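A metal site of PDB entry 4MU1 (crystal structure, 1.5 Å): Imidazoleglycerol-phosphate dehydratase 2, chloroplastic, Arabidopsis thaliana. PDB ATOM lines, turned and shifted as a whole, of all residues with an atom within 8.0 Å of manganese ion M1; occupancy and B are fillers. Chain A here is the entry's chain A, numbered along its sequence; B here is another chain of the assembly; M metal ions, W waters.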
ATOM      1  N   PHE A  56      22.406 -15.177 -12.259  1.00  0.00           N
ATOM      2  CA  PHE A  56      20.965 -14.935 -12.019  1.00  0.00           C
ATOM      3  C   PHE A  56      20.366 -16.062 -11.176  1.00  0.00           C
ATOM      4  O   PHE A  56      19.509 -15.840 -10.294  1.00  0.00           O
ATOM      5  CB  PHE A  56      20.164 -14.649 -13.315  1.00  0.00           C
ATOM      6  CG  PHE A  56      18.805 -14.060 -13.031  1.00  0.00           C
ATOM      7  CD1 PHE A  56      18.675 -12.699 -12.840  1.00  0.00           C
ATOM      8  CD2 PHE A  56      17.694 -14.871 -12.907  1.00  0.00           C
ATOM      9  CE1 PHE A  56      17.446 -12.132 -12.532  1.00  0.00           C
ATOM     10  CE2 PHE A  56      16.447 -14.311 -12.577  1.00  0.00           C
ATOM     11  CZ  PHE A  56      16.333 -12.952 -12.403  1.00  0.00           C
ATOM     12  N   HIS A  59      21.215 -15.657  -7.628  1.00  0.00           N
ATOM     13  CA  HIS A  59      20.340 -14.661  -7.059  1.00  0.00           C
ATOM     14  C   HIS A  59      18.967 -15.285  -6.677  1.00  0.00           C
ATOM     15  O   HIS A  59      18.404 -15.014  -5.608  1.00  0.00           O
ATOM     16  CB  HIS A  59      20.228 -13.495  -8.019  1.00  0.00           C
ATOM     17  CG  HIS A  59      19.325 -12.379  -7.593  1.00  0.00           C
ATOM     18  ND1 HIS A  59      19.299 -11.854  -6.318  1.00  0.00           N
ATOM     19  CD2 HIS A  59      18.469 -11.636  -8.325  1.00  0.00           C
ATOM     20  CE1 HIS A  59      18.435 -10.863  -6.273  1.00  0.00           C
ATOM     21  NE2 HIS A  59      17.925 -10.698  -7.483  1.00  0.00           N
ATOM     22  N   MET A  60      18.441 -16.125  -7.552  1.00  0.00           N
ATOM     23  CA  MET A  60      17.163 -16.766  -7.263  1.00  0.00           C
ATOM     24  C   MET A  60      17.256 -17.777  -6.101  1.00  0.00           C
ATOM     25  O   MET A  60      16.341 -17.936  -5.330  1.00  0.00           O
ATOM     26  CB  MET A  60      16.546 -17.422  -8.502  1.00  0.00           C
ATOM     27  CG  MET A  60      16.126 -16.453  -9.601  1.00  0.00           C
ATOM     28  SD  MET A  60      14.957 -15.175  -9.054  1.00  0.00           S
ATOM     29  CE  MET A  60      16.044 -13.769  -8.748  1.00  0.00           C
ATOM     30  N   GLN A  63      17.069 -15.977  -2.963  1.00  0.00           N
ATOM     31  CA  GLN A  63      15.647 -15.681  -2.689  1.00  0.00           C
ATOM     32  C   GLN A  63      14.953 -16.891  -2.026  1.00  0.00           C
ATOM     33  O   GLN A  63      14.121 -16.743  -1.121  1.00  0.00           O
ATOM     34  CB  GLN A  63      14.895 -15.261  -3.985  1.00  0.00           C
ATOM     35  CG  GLN A  63      15.356 -13.875  -4.473  1.00  0.00           C
ATOM     36  CD  GLN A  63      14.636 -12.799  -3.713  1.00  0.00           C
ATOM     37  OE1 GLN A  63      13.388 -12.815  -3.618  1.00  0.00           O
ATOM     38  NE2 GLN A  63      15.367 -11.864  -3.197  1.00  0.00           N
ATOM     39  N   LEU A 119       5.720  -8.699  -6.591  1.00  0.00           N
ATOM     40  CA  LEU A 119       6.939  -7.896  -6.658  1.00  0.00           C
ATOM     41  C   LEU A 119       6.585  -6.751  -7.589  1.00  0.00           C
ATOM     42  O   LEU A 119       6.484  -6.919  -8.827  1.00  0.00           O
ATOM     43  CB  LEU A 119       8.154  -8.679  -7.125  1.00  0.00           C
ATOM     44  CG  LEU A 119       9.501  -8.019  -6.845  1.00  0.00           C
ATOM     45  CD1 LEU A 119      10.648  -8.845  -7.421  1.00  0.00           C
ATOM     46  CD2 LEU A 119       9.648  -6.563  -7.164  1.00  0.00           C
ATOM     47  N   HIS A 181      12.529  -9.627 -14.748  1.00  0.00           N
ATOM     48  CA  HIS A 181      13.185  -9.863 -13.437  1.00  0.00           C
ATOM     49  C   HIS A 181      12.124  -9.933 -12.337  1.00  0.00           C
ATOM     50  O   HIS A 181      12.171 -10.830 -11.485  1.00  0.00           O
ATOM     51  CB  HIS A 181      14.261  -8.774 -13.259  1.00  0.00           C
ATOM     52  CG  HIS A 181      15.134  -8.875 -12.064  1.00  0.00           C
ATOM     53  ND1 HIS A 181      16.483  -8.573 -12.168  1.00  0.00           N
ATOM     54  CD2 HIS A 181      14.901  -9.120 -10.749  1.00  0.00           C
ATOM     55  CE1 HIS A 181      17.046  -8.646 -10.966  1.00  0.00           C
ATOM     56  NE2 HIS A 181      16.125  -9.019 -10.101  1.00  0.00           N
ATOM     57  N   HIS A 182      11.170  -9.022 -12.333  1.00  0.00           N
ATOM     58  CA  HIS A 182      10.104  -9.025 -11.320  1.00  0.00           C
ATOM     59  C   HIS A 182       9.303 -10.313 -11.389  1.00  0.00           C
ATOM     60  O   HIS A 182       8.964 -10.905 -10.354  1.00  0.00           O
ATOM     61  CB  HIS A 182       9.147  -7.850 -11.448  1.00  0.00           C
ATOM     62  CG  HIS A 182       9.768  -6.523 -11.103  1.00  0.00           C
ATOM     63  ND1 HIS A 182       9.110  -5.313 -11.276  1.00  0.00           N
ATOM     64  CD2 HIS A 182      10.975  -6.205 -10.573  1.00  0.00           C
ATOM     65  CE1 HIS A 182       9.873  -4.335 -10.854  1.00  0.00           C
ATOM     66  NE2 HIS A 182      11.004  -4.837 -10.418  1.00  0.00           N
ATOM     67  N   GLU A 185      11.546 -13.303 -10.127  1.00  0.00           N
ATOM     68  CA  GLU A 185      11.828 -13.161  -8.704  1.00  0.00           C
ATOM     69  C   GLU A 185      10.593 -13.362  -7.830  1.00  0.00           C
ATOM     70  O   GLU A 185      10.636 -14.049  -6.795  1.00  0.00           O
ATOM     71  CB  GLU A 185      12.542 -11.851  -8.415  1.00  0.00           C
ATOM     72  CG  GLU A 185      13.102 -11.777  -6.998  1.00  0.00           C
ATOM     73  CD  GLU A 185      13.939 -10.536  -6.782  1.00  0.00           C
ATOM     74  OE1 GLU A 185      14.741 -10.163  -7.703  1.00  0.00           O
ATOM     75  OE2 GLU A 185      13.762  -9.894  -5.692  1.00  0.00           O
ATOM     76  N   ALA A 186       9.468 -12.779  -8.231  1.00  0.00           N
ATOM     77  CA  ALA A 186       8.201 -13.027  -7.538  1.00  0.00           C
ATOM     78  C   ALA A 186       7.869 -14.523  -7.511  1.00  0.00           C
ATOM     79  O   ALA A 186       7.366 -15.033  -6.528  1.00  0.00           O
ATOM     80  CB  ALA A 186       7.053 -12.245  -8.162  1.00  0.00           C
ATOM     81  N   LYS A 189       9.929 -16.074  -4.800  1.00  0.00           N
ATOM     82  CA  LYS A 189       9.369 -15.681  -3.498  1.00  0.00           C
ATOM     83  C   LYS A 189       8.150 -16.524  -3.150  1.00  0.00           C
ATOM     84  O   LYS A 189       8.033 -17.032  -2.030  1.00  0.00           O
ATOM     85  CB  LYS A 189       8.962 -14.205  -3.435  1.00  0.00           C
ATOM     86  CG  LYS A 189      10.079 -13.177  -3.592  1.00  0.00           C
ATOM     87  CD  LYS A 189       9.548 -11.732  -3.502  1.00  0.00           C
ATOM     88  CE  LYS A 189      10.354 -10.738  -4.229  1.00  0.00           C
ATOM     89  NZ  LYS A 189      11.699 -10.669  -3.654  1.00  0.00           N
ATOM     90  N   GLU B  33      22.970  -4.697  -2.417  1.00  0.00           N
ATOM     91  CA  GLU B  33      23.131  -4.844  -3.868  1.00  0.00           C
ATOM     92  C   GLU B  33      23.958  -3.719  -4.513  1.00  0.00           C
ATOM     93  O   GLU B  33      24.640  -3.924  -5.534  1.00  0.00           O
ATOM     94  CB  GLU B  33      21.755  -4.891  -4.570  1.00  0.00           C
ATOM     95  CG  GLU B  33      20.955  -6.155  -4.275  1.00  0.00           C
ATOM     96  CD  GLU B  33      20.053  -6.065  -3.064  1.00  0.00           C
ATOM     97  OE1 GLU B  33      20.079  -5.051  -2.348  1.00  0.00           O
ATOM     98  OE2 GLU B  33      19.299  -7.031  -2.831  1.00  0.00           O
ATOM     99  N   ASP B  79      25.650  -4.849  -8.359  1.00  0.00           N
ATOM    100  CA  ASP B  79      25.680  -6.262  -8.779  1.00  0.00           C
ATOM    101  C   ASP B  79      25.304  -6.481 -10.258  1.00  0.00           C
ATOM    102  O   ASP B  79      24.445  -7.281 -10.596  1.00  0.00           O
ATOM    103  CB  ASP B  79      24.814  -7.125  -7.822  1.00  0.00           C
ATOM    104  CG  ASP B  79      23.355  -6.674  -7.731  1.00  0.00           C
ATOM    105  OD1 ASP B  79      22.920  -5.754  -8.473  1.00  0.00           O
ATOM    106  OD2 ASP B  79      22.629  -7.256  -6.893  1.00  0.00           O
ATOM    107  N   ILE B  82      24.667  -9.857 -12.172  1.00  0.00           N
ATOM    108  CA  ILE B  82      23.321 -10.488 -12.117  1.00  0.00           C
ATOM    109  C   ILE B  82      22.510  -9.903 -13.281  1.00  0.00           C
ATOM    110  O   ILE B  82      21.992 -10.618 -14.126  1.00  0.00           O
ATOM    111  CB  ILE B  82      22.593 -10.211 -10.783  1.00  0.00           C
ATOM    112  CG1 ILE B  82      23.308 -10.879  -9.609  1.00  0.00           C
ATOM    113  CG2 ILE B  82      21.137 -10.678 -10.881  1.00  0.00           C
ATOM    114  CD1 ILE B  82      22.800 -10.516  -8.242  1.00  0.00           C
ATOM    115  N   ASP B  83      22.381  -8.586 -13.275  1.00  0.00           N
ATOM    116  CA  ASP B  83      21.910  -7.784 -14.429  1.00  0.00           C
ATOM    117  C   ASP B  83      22.000  -6.318 -13.965  1.00  0.00           C
ATOM    118  O   ASP B  83      22.447  -6.030 -12.850  1.00  0.00           O
ATOM    119  CB  ASP B  83      20.499  -8.218 -14.940  1.00  0.00           C
ATOM    120  CG  ASP B  83      19.356  -7.873 -14.004  1.00  0.00           C
ATOM    121  OD1 ASP B  83      19.596  -7.365 -12.887  1.00  0.00           O
ATOM    122  OD2 ASP B  83      18.140  -8.105 -14.419  1.00  0.00           O
ATOM    123  N   HIS B  85      19.506  -4.350 -13.305  1.00  0.00           N
ATOM    124  CA  HIS B  85      18.231  -3.961 -12.663  1.00  0.00           C
ATOM    125  C   HIS B  85      18.414  -3.238 -11.335  1.00  0.00           C
ATOM    126  O   HIS B  85      17.842  -2.144 -11.130  1.00  0.00           O
ATOM    127  CB  HIS B  85      17.380  -5.209 -12.435  1.00  0.00           C
ATOM    128  CG  HIS B  85      15.976  -4.922 -11.997  1.00  0.00           C
ATOM    129  ND1 HIS B  85      14.856  -5.240 -12.750  1.00  0.00           N
ATOM    130  CD2 HIS B  85      15.502  -4.394 -10.834  1.00  0.00           C
ATOM    131  CE1 HIS B  85      13.762  -4.912 -12.076  1.00  0.00           C
ATOM    132  NE2 HIS B  85      14.120  -4.404 -10.904  1.00  0.00           N
ATOM    133  N   HIS B  86      19.173  -3.838 -10.420  1.00  0.00           N
ATOM    134  CA  HIS B  86      19.234  -3.249  -9.094  1.00  0.00           C
ATOM    135  C   HIS B  86      19.945  -1.888  -9.107  1.00  0.00           C
ATOM    136  O   HIS B  86      19.551  -0.957  -8.422  1.00  0.00           O
ATOM    137  CB  HIS B  86      19.858  -4.177  -8.038  1.00  0.00           C
ATOM    138  CG  HIS B  86      19.256  -5.544  -7.943  1.00  0.00           C
ATOM    139  ND1 HIS B  86      19.975  -6.628  -7.494  1.00  0.00           N
ATOM    140  CD2 HIS B  86      17.993  -5.981  -8.146  1.00  0.00           C
ATOM    141  CE1 HIS B  86      19.189  -7.694  -7.470  1.00  0.00           C
ATOM    142  NE2 HIS B  86      17.975  -7.322  -7.872  1.00  0.00           N
ATOM    143  N   GLU B  89      17.628   0.787 -10.685  1.00  0.00           N
ATOM    144  CA  GLU B  89      16.555   1.107  -9.732  1.00  0.00           C
ATOM    145  C   GLU B  89      17.105   2.027  -8.625  1.00  0.00           C
ATOM    146  O   GLU B  89      16.502   3.068  -8.267  1.00  0.00           O
ATOM    147  CB  GLU B  89      15.994  -0.169  -9.115  1.00  0.00           C
ATOM    148  CG  GLU B  89      14.909   0.100  -8.094  1.00  0.00           C
ATOM    149  CD  GLU B  89      14.014  -1.100  -7.801  1.00  0.00           C
ATOM    150  OE1 GLU B  89      14.203  -2.142  -8.496  1.00  0.00           O
ATOM    151  OE2 GLU B  89      13.077  -0.913  -6.961  1.00  0.00           O
HETATM  152 MN    MN M   1      16.525  -9.098  -7.925  1.00  0.00          MN
HETATM  153 MN    MN M   2      12.677  -3.588  -9.401  1.00  0.00          MN
HETATM  154  O   HOH W   1      16.302  -8.628  -5.668  1.00  0.00           O
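The side-chain carboxylate of Glu 185 is in salt-bridge range of the side-chain amino group of Lys 189 (3.0 Å).
A ring nitrogen (ND1) of His 86 of chain B lies within hydrogen-bond range of the side-chain carboxylate (OD2) of Asp 79 of chain B.
ND1 of His 181 sits at hydrogen-bond distance from OD2 of Asp 83 of chain B (2.8 Å).
Four residues have an atom within 4 Å of manganese ion M1: His 59, His 181, Glu 185 and His 86 of chain B.
Manganese ion M1 is bound by OE1 of Glu 185 (2.1 Å).
Manganese ion M1 is bound by NE2 of His 59 (2.2 Å).
A ring nitrogen (NE2) of His 181 is bound to manganese ion M1, at 2.2 Å.
Manganese ion M1 is bound by a ring nitrogen (NE2) of His 86 of chain B.
Water W1 is bound to manganese ion M1 (2.3 Å).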
